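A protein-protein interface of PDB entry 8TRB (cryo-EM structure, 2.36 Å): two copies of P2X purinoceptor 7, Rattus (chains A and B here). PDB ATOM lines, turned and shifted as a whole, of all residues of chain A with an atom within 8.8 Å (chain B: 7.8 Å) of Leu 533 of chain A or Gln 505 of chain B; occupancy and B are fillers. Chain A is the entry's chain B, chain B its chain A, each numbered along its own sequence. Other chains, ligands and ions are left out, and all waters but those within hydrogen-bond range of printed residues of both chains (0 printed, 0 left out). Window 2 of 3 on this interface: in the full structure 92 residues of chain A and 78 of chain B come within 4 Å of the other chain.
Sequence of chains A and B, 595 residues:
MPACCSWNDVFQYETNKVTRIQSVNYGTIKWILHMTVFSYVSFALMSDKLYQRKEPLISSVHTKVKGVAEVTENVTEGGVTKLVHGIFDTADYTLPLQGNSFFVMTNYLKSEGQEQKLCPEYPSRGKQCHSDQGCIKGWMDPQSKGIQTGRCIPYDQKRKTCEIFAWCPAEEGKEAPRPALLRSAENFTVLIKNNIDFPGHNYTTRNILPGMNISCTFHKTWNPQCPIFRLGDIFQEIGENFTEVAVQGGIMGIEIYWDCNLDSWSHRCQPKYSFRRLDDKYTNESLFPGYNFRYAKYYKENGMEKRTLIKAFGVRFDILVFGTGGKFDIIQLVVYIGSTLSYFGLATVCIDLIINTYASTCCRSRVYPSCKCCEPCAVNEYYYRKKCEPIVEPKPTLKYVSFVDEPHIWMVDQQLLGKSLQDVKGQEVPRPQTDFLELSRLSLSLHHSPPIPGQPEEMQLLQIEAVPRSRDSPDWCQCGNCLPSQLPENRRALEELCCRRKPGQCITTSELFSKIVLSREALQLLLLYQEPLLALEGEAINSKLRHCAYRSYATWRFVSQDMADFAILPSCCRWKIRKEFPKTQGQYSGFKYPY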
ATOM      1  N   LEU A 527     -33.236  16.519   8.622  1.00  0.00           N
ATOM      2  CA  LEU A 527     -33.197  15.597   7.495  1.00  0.00           C
ATOM      3  C   LEU A 527     -31.806  15.554   6.879  1.00  0.00           C
ATOM      4  O   LEU A 527     -31.279  14.476   6.580  1.00  0.00           O
ATOM      5  CB  LEU A 527     -34.228  16.017   6.448  1.00  0.00           C
ATOM      6  CG  LEU A 527     -35.563  15.274   6.436  1.00  0.00           C
ATOM      7  CD1 LEU A 527     -36.101  15.117   7.833  1.00  0.00           C
ATOM      8  CD2 LEU A 527     -36.567  16.014   5.575  1.00  0.00           C
ATOM      9  N   LEU A 528     -31.200  16.723   6.683  1.00  0.00           N
ATOM     10  CA  LEU A 528     -29.855  16.780   6.123  1.00  0.00           C
ATOM     11  C   LEU A 528     -28.851  16.111   7.052  1.00  0.00           C
ATOM     12  O   LEU A 528     -27.954  15.394   6.597  1.00  0.00           O
ATOM     13  CB  LEU A 528     -29.463  18.232   5.869  1.00  0.00           C
ATOM     14  CG  LEU A 528     -30.276  18.964   4.806  1.00  0.00           C
ATOM     15  CD1 LEU A 528     -29.917  20.438   4.792  1.00  0.00           C
ATOM     16  CD2 LEU A 528     -30.060  18.342   3.448  1.00  0.00           C
ATOM     17  N   TYR A 529     -28.993  16.335   8.356  1.00  0.00           N
ATOM     18  CA  TYR A 529     -28.112  15.685   9.319  1.00  0.00           C
ATOM     19  C   TYR A 529     -28.204  14.172   9.196  1.00  0.00           C
ATOM     20  O   TYR A 529     -27.185  13.475   9.202  1.00  0.00           O
ATOM     21  CB  TYR A 529     -28.475  16.134  10.733  1.00  0.00           C
ATOM     22  CG  TYR A 529     -27.396  15.899  11.756  1.00  0.00           C
ATOM     23  CD1 TYR A 529     -27.287  14.683  12.407  1.00  0.00           C
ATOM     24  CD2 TYR A 529     -26.490  16.894  12.074  1.00  0.00           C
ATOM     25  CE1 TYR A 529     -26.304  14.466  13.343  1.00  0.00           C
ATOM     26  CE2 TYR A 529     -25.506  16.688  13.008  1.00  0.00           C
ATOM     27  CZ  TYR A 529     -25.416  15.472  13.639  1.00  0.00           C
ATOM     28  OH  TYR A 529     -24.431  15.268  14.572  1.00  0.00           O
ATOM     29  N   GLN A 530     -29.425  13.648   9.082  1.00  0.00           N
ATOM     30  CA  GLN A 530     -29.593  12.215   8.877  1.00  0.00           C
ATOM     31  C   GLN A 530     -29.197  11.810   7.462  1.00  0.00           C
ATOM     32  O   GLN A 530     -28.503  10.802   7.273  1.00  0.00           O
ATOM     33  CB  GLN A 530     -31.039  11.817   9.167  1.00  0.00           C
ATOM     34  CG  GLN A 530     -31.246  10.324   9.314  1.00  0.00           C
ATOM     35  CD  GLN A 530     -30.568   9.766  10.547  1.00  0.00           C
ATOM     36  OE1 GLN A 530     -30.518  10.417  11.590  1.00  0.00           O
ATOM     37  NE2 GLN A 530     -30.035   8.556  10.429  1.00  0.00           N
ATOM     38  N   GLU A 531     -29.623  12.578   6.459  1.00  0.00           N
ATOM     39  CA  GLU A 531     -29.357  12.281   5.054  1.00  0.00           C
ATOM     40  C   GLU A 531     -28.813  13.540   4.388  1.00  0.00           C
ATOM     41  O   GLU A 531     -29.580  14.365   3.878  1.00  0.00           O
ATOM     42  CB  GLU A 531     -30.618  11.789   4.349  1.00  0.00           C
ATOM     43  CG  GLU A 531     -30.892  10.304   4.543  1.00  0.00           C
ATOM     44  CD  GLU A 531     -32.339   9.933   4.277  1.00  0.00           C
ATOM     45  OE1 GLU A 531     -33.226  10.782   4.505  1.00  0.00           O
ATOM     46  OE2 GLU A 531     -32.591   8.790   3.842  1.00  0.00           O
ATOM     47  N   PRO A 532     -27.488  13.719   4.373  1.00  0.00           N
ATOM     48  CA  PRO A 532     -26.934  14.984   3.856  1.00  0.00           C
ATOM     49  C   PRO A 532     -27.336  15.294   2.427  1.00  0.00           C
ATOM     50  O   PRO A 532     -27.548  16.467   2.092  1.00  0.00           O
ATOM     51  CB  PRO A 532     -25.420  14.777   3.984  1.00  0.00           C
ATOM     52  CG  PRO A 532     -25.250  13.681   4.964  1.00  0.00           C
ATOM     53  CD  PRO A 532     -26.437  12.803   4.841  1.00  0.00           C
ATOM     54  N   LEU A 533     -27.445  14.283   1.566  1.00  0.00           N
ATOM     55  CA  LEU A 533     -27.786  14.483   0.164  1.00  0.00           C
ATOM     56  C   LEU A 533     -29.252  14.177  -0.120  1.00  0.00           C
ATOM     57  O   LEU A 533     -29.587  13.706  -1.213  1.00  0.00           O
ATOM     58  CB  LEU A 533     -26.889  13.625  -0.724  1.00  0.00           C
ATOM     59  CG  LEU A 533     -25.385  13.784  -0.514  1.00  0.00           C
ATOM     60  CD1 LEU A 533     -24.640  12.816  -1.410  1.00  0.00           C
ATOM     61  CD2 LEU A 533     -24.932  15.206  -0.772  1.00  0.00           C
ATOM     62  N   LEU A 534     -30.129  14.431   0.843  1.00  0.00           N
ATOM     63  CA  LEU A 534     -31.547  14.185   0.645  1.00  0.00           C
ATOM     64  C   LEU A 534     -32.107  15.140  -0.401  1.00  0.00           C
ATOM     65  O   LEU A 534     -31.800  16.336  -0.401  1.00  0.00           O
ATOM     66  CB  LEU A 534     -32.300  14.349   1.963  1.00  0.00           C
ATOM     67  CG  LEU A 534     -33.731  13.818   2.004  1.00  0.00           C
ATOM     68  CD1 LEU A 534     -33.757  12.312   1.791  1.00  0.00           C
ATOM     69  CD2 LEU A 534     -34.390  14.187   3.319  1.00  0.00           C
ATOM     70  N   ALA A 535     -32.933  14.606  -1.295  1.00  0.00           N
ATOM     71  CA  ALA A 535     -33.563  15.396  -2.343  1.00  0.00           C
ATOM     72  C   ALA A 535     -34.905  15.914  -1.840  1.00  0.00           C
ATOM     73  O   ALA A 535     -35.819  15.128  -1.570  1.00  0.00           O
ATOM     74  CB  ALA A 535     -33.748  14.563  -3.608  1.00  0.00           C
ATOM     75  N   LEU A 536     -35.020  17.236  -1.718  1.00  0.00           N
ATOM     76  CA  LEU A 536     -36.239  17.864  -1.205  1.00  0.00           C
ATOM     77  C   LEU A 536     -37.232  18.058  -2.351  1.00  0.00           C
ATOM     78  O   LEU A 536     -37.540  19.170  -2.785  1.00  0.00           O
ATOM     79  CB  LEU A 536     -35.907  19.182  -0.519  1.00  0.00           C
ATOM     80  CG  LEU A 536     -34.663  19.178   0.373  1.00  0.00           C
ATOM     81  CD1 LEU A 536     -34.557  20.488   1.134  1.00  0.00           C
ATOM     82  CD2 LEU A 536     -34.676  17.998   1.329  1.00  0.00           C
ATOM     83  N   PHE B 403     -19.518   6.477   3.971  1.00  0.00           N
ATOM     84  CA  PHE B 403     -19.837   6.897   2.616  1.00  0.00           C
ATOM     85  C   PHE B 403     -21.260   7.430   2.577  1.00  0.00           C
ATOM     86  O   PHE B 403     -22.195   6.754   3.016  1.00  0.00           O
ATOM     87  CB  PHE B 403     -19.660   5.738   1.640  1.00  0.00           C
ATOM     88  CG  PHE B 403     -18.273   5.178   1.626  1.00  0.00           C
ATOM     89  CD1 PHE B 403     -17.219   5.922   1.140  1.00  0.00           C
ATOM     90  CD2 PHE B 403     -18.019   3.918   2.121  1.00  0.00           C
ATOM     91  CE1 PHE B 403     -15.947   5.415   1.134  1.00  0.00           C
ATOM     92  CE2 PHE B 403     -16.746   3.408   2.115  1.00  0.00           C
ATOM     93  CZ  PHE B 403     -15.710   4.158   1.622  1.00  0.00           C
ATOM     94  N   VAL B 404     -21.411   8.646   2.055  1.00  0.00           N
ATOM     95  CA  VAL B 404     -22.711   9.308   2.055  1.00  0.00           C
ATOM     96  C   VAL B 404     -23.719   8.498   1.254  1.00  0.00           C
ATOM     97  O   VAL B 404     -24.904   8.431   1.604  1.00  0.00           O
ATOM     98  CB  VAL B 404     -22.563  10.743   1.523  1.00  0.00           C
ATOM     99  CG1 VAL B 404     -22.258  10.735   0.045  1.00  0.00           C
ATOM    100  CG2 VAL B 404     -23.804  11.550   1.817  1.00  0.00           C
ATOM    101  N   ASP B 405     -23.270   7.870   0.168  1.00  0.00           N
ATOM    102  CA  ASP B 405     -24.159   7.020  -0.615  1.00  0.00           C
ATOM    103  C   ASP B 405     -24.660   5.841   0.209  1.00  0.00           C
ATOM    104  O   ASP B 405     -25.838   5.471   0.129  1.00  0.00           O
ATOM    105  CB  ASP B 405     -23.440   6.536  -1.873  1.00  0.00           C
ATOM    106  CG  ASP B 405     -22.170   5.775  -1.564  1.00  0.00           C
ATOM    107  OD1 ASP B 405     -21.132   6.424  -1.323  1.00  0.00           O
ATOM    108  OD2 ASP B 405     -22.208   4.526  -1.566  1.00  0.00           O
ATOM    109  N   GLN B 478     -14.591   9.699  -6.387  1.00  0.00           N
ATOM    110  CA  GLN B 478     -15.859   9.558  -7.092  1.00  0.00           C
ATOM    111  C   GLN B 478     -16.710  10.818  -6.966  1.00  0.00           C
ATOM    112  O   GLN B 478     -17.932  10.747  -7.141  1.00  0.00           O
ATOM    113  CB  GLN B 478     -16.664   8.364  -6.573  1.00  0.00           C
ATOM    114  CG  GLN B 478     -15.846   7.146  -6.173  1.00  0.00           C
ATOM    115  CD  GLN B 478     -15.522   6.242  -7.340  1.00  0.00           C
ATOM    116  OE1 GLN B 478     -16.069   6.390  -8.432  1.00  0.00           O
ATOM    117  NE2 GLN B 478     -14.621   5.292  -7.113  1.00  0.00           N
ATOM    118  N   CYS B 479     -16.104  11.961  -6.650  1.00  0.00           N
ATOM    119  CA  CYS B 479     -16.865  13.189  -6.467  1.00  0.00           C
ATOM    120  C   CYS B 479     -16.230  14.416  -7.100  1.00  0.00           C
ATOM    121  O   CYS B 479     -16.877  15.465  -7.128  1.00  0.00           O
ATOM    122  CB  CYS B 479     -17.092  13.456  -4.971  1.00  0.00           C
ATOM    123  SG  CYS B 479     -15.613  13.845  -4.013  1.00  0.00           S
ATOM    124  N   GLY B 480     -15.000  14.335  -7.603  1.00  0.00           N
ATOM    125  CA  GLY B 480     -14.387  15.449  -8.293  1.00  0.00           C
ATOM    126  C   GLY B 480     -13.789  16.511  -7.401  1.00  0.00           C
ATOM    127  O   GLY B 480     -13.416  17.576  -7.903  1.00  0.00           O
ATOM    128  N   ASN B 481     -13.685  16.259  -6.096  1.00  0.00           N
ATOM    129  CA  ASN B 481     -13.126  17.219  -5.157  1.00  0.00           C
ATOM    130  C   ASN B 481     -11.950  16.681  -4.365  1.00  0.00           C
ATOM    131  O   ASN B 481     -11.229  17.474  -3.752  1.00  0.00           O
ATOM    132  CB  ASN B 481     -14.204  17.689  -4.168  1.00  0.00           C
ATOM    133  CG  ASN B 481     -15.453  18.185  -4.860  1.00  0.00           C
ATOM    134  OD1 ASN B 481     -16.138  17.429  -5.548  1.00  0.00           O
ATOM    135  ND2 ASN B 481     -15.760  19.461  -4.681  1.00  0.00           N
ATOM    136  N   CYS B 499     -15.491  10.600  -0.249  1.00  0.00           N
ATOM    137  CA  CYS B 499     -16.718  10.735   0.518  1.00  0.00           C
ATOM    138  C   CYS B 499     -17.787   9.732   0.115  1.00  0.00           C
ATOM    139  O   CYS B 499     -18.752   9.553   0.864  1.00  0.00           O
ATOM    140  CB  CYS B 499     -17.257  12.157   0.371  1.00  0.00           C
ATOM    141  SG  CYS B 499     -17.828  12.580  -1.281  1.00  0.00           S
ATOM    142  N   ARG B 500     -17.645   9.073  -1.033  1.00  0.00           N
ATOM    143  CA  ARG B 500     -18.647   8.131  -1.501  1.00  0.00           C
ATOM    144  C   ARG B 500     -17.964   7.019  -2.281  1.00  0.00           C
ATOM    145  O   ARG B 500     -16.879   7.207  -2.838  1.00  0.00           O
ATOM    146  CB  ARG B 500     -19.695   8.821  -2.374  1.00  0.00           C
ATOM    147  CG  ARG B 500     -19.110   9.646  -3.505  1.00  0.00           C
ATOM    148  CD  ARG B 500     -20.173  10.448  -4.218  1.00  0.00           C
ATOM    149  NE  ARG B 500     -21.444   9.731  -4.274  1.00  0.00           N
ATOM    150  CZ  ARG B 500     -22.635  10.277  -4.050  1.00  0.00           C
ATOM    151  NH1 ARG B 500     -22.751  11.564  -3.753  1.00  0.00           N
ATOM    152  NH2 ARG B 500     -23.720   9.524  -4.125  1.00  0.00           N
ATOM    153  N   LYS B 502     -19.457   5.420  -4.944  1.00  0.00           N
ATOM    154  CA  LYS B 502     -19.870   5.517  -6.333  1.00  0.00           C
ATOM    155  C   LYS B 502     -19.964   6.973  -6.764  1.00  0.00           C
ATOM    156  O   LYS B 502     -20.115   7.870  -5.925  1.00  0.00           O
ATOM    157  CB  LYS B 502     -21.226   4.831  -6.544  1.00  0.00           C
ATOM    158  CG  LYS B 502     -21.208   3.335  -6.290  1.00  0.00           C
ATOM    159  CD  LYS B 502     -22.602   2.803  -6.025  1.00  0.00           C
ATOM    160  CE  LYS B 502     -22.560   1.382  -5.490  1.00  0.00           C
ATOM    161  NZ  LYS B 502     -23.872   0.689  -5.620  1.00  0.00           N
ATOM    162  N   PRO B 503     -19.889   7.245  -8.066  1.00  0.00           N
ATOM    163  CA  PRO B 503     -19.925   8.636  -8.530  1.00  0.00           C
ATOM    164  C   PRO B 503     -21.205   9.338  -8.105  1.00  0.00           C
ATOM    165  O   PRO B 503     -22.283   8.743  -8.069  1.00  0.00           O
ATOM    166  CB  PRO B 503     -19.830   8.508 -10.054  1.00  0.00           C
ATOM    167  CG  PRO B 503     -19.241   7.168 -10.295  1.00  0.00           C
ATOM    168  CD  PRO B 503     -19.721   6.299  -9.182  1.00  0.00           C
ATOM    169  N   GLY B 504     -21.072  10.619  -7.784  1.00  0.00           N
ATOM    170  CA  GLY B 504     -22.207  11.398  -7.345  1.00  0.00           C
ATOM    171  C   GLY B 504     -21.758  12.754  -6.838  1.00  0.00           C
ATOM    172  O   GLY B 504     -20.592  13.133  -6.971  1.00  0.00           O
ATOM    173  N   GLN B 505     -22.712  13.477  -6.262  1.00  0.00           N
ATOM    174  CA  GLN B 505     -22.418  14.790  -5.709  1.00  0.00           C
ATOM    175  C   GLN B 505     -21.621  14.656  -4.418  1.00  0.00           C
ATOM    176  O   GLN B 505     -21.858  13.757  -3.609  1.00  0.00           O
ATOM    177  CB  GLN B 505     -23.713  15.563  -5.453  1.00  0.00           C
ATOM    178  CG  GLN B 505     -24.690  14.861  -4.532  1.00  0.00           C
ATOM    179  CD  GLN B 505     -25.931  15.683  -4.263  1.00  0.00           C
ATOM    180  OE1 GLN B 505     -25.879  16.912  -4.217  1.00  0.00           O
ATOM    181  NE2 GLN B 505     -27.059  15.006  -4.077  1.00  0.00           N
ATOM    182  N   CYS B 506     -20.662  15.558  -4.234  1.00  0.00           N
ATOM    183  CA  CYS B 506     -19.848  15.540  -3.033  1.00  0.00           C
ATOM    184  C   CYS B 506     -20.665  15.963  -1.818  1.00  0.00           C
ATOM    185  O   CYS B 506     -21.576  16.788  -1.905  1.00  0.00           O
ATOM    186  CB  CYS B 506     -18.646  16.467  -3.182  1.00  0.00           C
ATOM    187  SG  CYS B 506     -17.457  16.340  -1.836  1.00  0.00           S
ATOM    188  N   ILE B 507     -20.320  15.376  -0.670  1.00  0.00           N
ATOM    189  CA  ILE B 507     -20.950  15.761   0.585  1.00  0.00           C
ATOM    190  C   ILE B 507     -20.641  17.213   0.920  1.00  0.00           C
ATOM    191  O   ILE B 507     -21.418  17.877   1.617  1.00  0.00           O
ATOM    192  CB  ILE B 507     -20.491  14.813   1.708  1.00  0.00           C
ATOM    193  CG1 ILE B 507     -21.428  14.909   2.908  1.00  0.00           C
ATOM    194  CG2 ILE B 507     -19.076  15.138   2.118  1.00  0.00           C
ATOM    195  CD1 ILE B 507     -21.105  13.932   3.996  1.00  0.00           C
ATOM    196  N   THR B 508     -19.509  17.727   0.438  1.00  0.00           N
ATOM    197  CA  THR B 508     -19.147  19.110   0.717  1.00  0.00           C
ATOM    198  C   THR B 508     -20.176  20.085   0.165  1.00  0.00           C
ATOM    199  O   THR B 508     -20.339  21.186   0.702  1.00  0.00           O
ATOM    200  CB  THR B 508     -17.771  19.424   0.133  1.00  0.00           C
ATOM    201  OG1 THR B 508     -17.730  19.026  -1.242  1.00  0.00           O
ATOM    202  CG2 THR B 508     -16.690  18.699   0.897  1.00  0.00           C
ATOM    203  N   THR B 509     -20.874  19.704  -0.904  1.00  0.00           N
ATOM    204  CA  THR B 509     -21.858  20.588  -1.510  1.00  0.00           C
ATOM    205  C   THR B 509     -23.121  20.711  -0.672  1.00  0.00           C
ATOM    206  O   THR B 509     -23.933  21.607  -0.923  1.00  0.00           O
ATOM    207  CB  THR B 509     -22.214  20.091  -2.911  1.00  0.00           C
ATOM    208  OG1 THR B 509     -22.881  18.825  -2.821  1.00  0.00           O
ATOM    209  CG2 THR B 509     -20.954  19.940  -3.753  1.00  0.00           C
ATOM    210  N   SER B 510     -23.311  19.832   0.308  1.00  0.00           N
ATOM    211  CA  SER B 510     -24.479  19.917   1.169  1.00  0.00           C
ATOM    212  C   SER B 510     -24.441  21.198   1.993  1.00  0.00           C
ATOM    213  O   SER B 510     -23.374  21.688   2.373  1.00  0.00           O
ATOM    214  CB  SER B 510     -24.551  18.701   2.090  1.00  0.00           C
ATOM    215  OG  SER B 510     -23.362  18.567   2.845  1.00  0.00           O
ATOM    216  N   GLU B 511     -25.627  21.744   2.264  1.00  0.00           N
ATOM    217  CA  GLU B 511     -25.708  22.983   3.032  1.00  0.00           C
ATOM    218  C   GLU B 511     -25.197  22.780   4.450  1.00  0.00           C
ATOM    219  O   GLU B 511     -24.535  23.658   5.013  1.00  0.00           O
ATOM    220  CB  GLU B 511     -27.148  23.494   3.047  1.00  0.00           C
ATOM    221  N   TRP B 556     -20.667  14.179  13.243  1.00  0.00           N
ATOM    222  CA  TRP B 556     -21.853  14.225  12.395  1.00  0.00           C
ATOM    223  C   TRP B 556     -22.016  12.938  11.596  1.00  0.00           C
ATOM    224  O   TRP B 556     -23.126  12.402  11.495  1.00  0.00           O
ATOM    225  CB  TRP B 556     -21.767  15.439  11.467  1.00  0.00           C
ATOM    226  CG  TRP B 556     -22.765  15.455  10.346  1.00  0.00           C
ATOM    227  CD1 TRP B 556     -24.038  14.962  10.365  1.00  0.00           C
ATOM    228  CD2 TRP B 556     -22.570  16.006   9.038  1.00  0.00           C
ATOM    229  NE1 TRP B 556     -24.644  15.166   9.149  1.00  0.00           N
ATOM    230  CE2 TRP B 556     -23.763  15.806   8.317  1.00  0.00           C
ATOM    231  CE3 TRP B 556     -21.500  16.647   8.406  1.00  0.00           C
ATOM    232  CZ2 TRP B 556     -23.916  16.224   6.998  1.00  0.00           C
ATOM    233  CZ3 TRP B 556     -21.654  17.061   7.096  1.00  0.00           C
ATOM    234  CH2 TRP B 556     -22.853  16.848   6.405  1.00  0.00           C
ATOM    235  N   ARG B 557     -20.928  12.421  11.029  1.00  0.00           N
ATOM    236  CA  ARG B 557     -21.007  11.254  10.158  1.00  0.00           C
ATOM    237  C   ARG B 557     -20.792   9.934  10.888  1.00  0.00           C
ATOM    238  O   ARG B 557     -20.891   8.876  10.259  1.00  0.00           O
ATOM    239  CB  ARG B 557     -19.990  11.381   9.020  1.00  0.00           C
ATOM    240  CG  ARG B 557     -20.168  12.626   8.162  1.00  0.00           C
ATOM    241  CD  ARG B 557     -21.568  12.724   7.576  1.00  0.00           C
ATOM    242  NE  ARG B 557     -21.975  11.490   6.911  1.00  0.00           N
ATOM    243  CZ  ARG B 557     -23.191  10.961   6.966  1.00  0.00           C
ATOM    244  NH1 ARG B 557     -24.169  11.537   7.646  1.00  0.00           N
ATOM    245  NH2 ARG B 557     -23.431   9.824   6.320  1.00  0.00           N
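The indole nitrogen of Trp 556 of chain B is in hydrogen-bond range of the backbone carbonyl oxygen of Tyr 529 of chain A (3.1 Å).
SG of Cys 506 of chain B sits close to OG1 of Thr 508 of chain B (2.8 Å).
O of Cys 506 of chain B lies within hydrogen-bond range of OG1 of Thr 509 of chain B (2.6 Å).
The backbone NH (N) of Val 404 of chain B sits at hydrogen-bond distance from the backbone carbonyl oxygen (O) of Cys 499 of chain B, at 3.1 Å.
The guanidinium group of Arg 500 of chain B is in hydrogen-bond range of the backbone carbonyl oxygen of Lys 502 of chain B, at 2.8 Å.
O of Ile 507 of chain B is in hydrogen-bond range of OG of Ser 510 of chain B, 2.4 Å away.
Arg 557 of chain B touches Tyr 529 of chain A (NH1 to O, 3.9 Å).
Pro 532 of chain A touches Ser 510 of chain B.
Trp 556 of chain B touches Pro 532 of chain A (CZ2 to CG, 3.5 Å).
Pro 532 of chain A touches Arg 557 of chain B (CG to NH1, 3.6 Å).
CG1 of Val 404 of chain B touches CD1 of Leu 533 of chain A, at 3.5 Å.
NH1 of Arg 500 of chain B touches CD1 of Leu 533 of chain A, at 3.3 Å.
Leu 533 of chain A touches Gln 505 of chain B (CB to NE2, 3.6 Å).
CD2 of Leu 533 of chain A touches O of Cys 506 of chain B, at 3.9 Å.
Printed residues of chain B within 4 Å of Leu 533 of chain A: Val 404, Arg 500, Gln 505 and Cys 506.
Gln 505 of chain B touches one residue of chain A.
Of the printed residues of chain B, Tyr 529 of chain A touches Trp 556 (3.1 Å) and Arg 557 (3.9 Å).
Of the printed residues of chain A, Arg 557 of chain B touches Tyr 529 (3.9 Å) and Pro 532 (3.6 Å).
Of the printed residues of chain A, Ser 510 of chain B touches Pro 532 (3.7 Å).
Of the printed residues of chain A, Val 404 of chain B touches Leu 533 (3.5 Å).
Ile 507 of chain B touches none of the printed residues of chain A.
Asp 405 of chain B touches none of the printed residues of chain A.
The nearest residue of chain B that does not touch Leu 533 of chain A is Ile 507 of chain B (4.2 Å).
The nearest residue of chain A that does not touch Gln 505 of chain B is Leu 534 of chain A (5.8 Å).
The nearest printed residue of chain A that does not touch Arg 557 of chain B is Gln 530 of chain A (4.4 Å).
Printed residues of chain B that touch a printed residue of chain A: Val 404, Arg 500, Gln 505, Cys 506, Ser 510, Trp 556 and Arg 557.
Of the 10 printed residues of chain A, 3 touch a printed residue of chain B.
Printed residues of chain A that touch a printed residue of chain B: Tyr 529, Pro 532 and Leu 533.
Hydrophobic or aromatic side chains of chain A that line the printed part of chain B: Tyr 529, Pro 532 and Leu 533.
Among the printed residues, 9 pairs touch across the chains.
Among the printed residues, no Asp or Glu carboxylate lies within 4 Å of a Lys or Arg side-chain nitrogen of the other chain.
No position is printed for both chains.
Of the 9 pairs that touch across the chains among the printed residues, none has its exchanged pair printed and touching as well.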
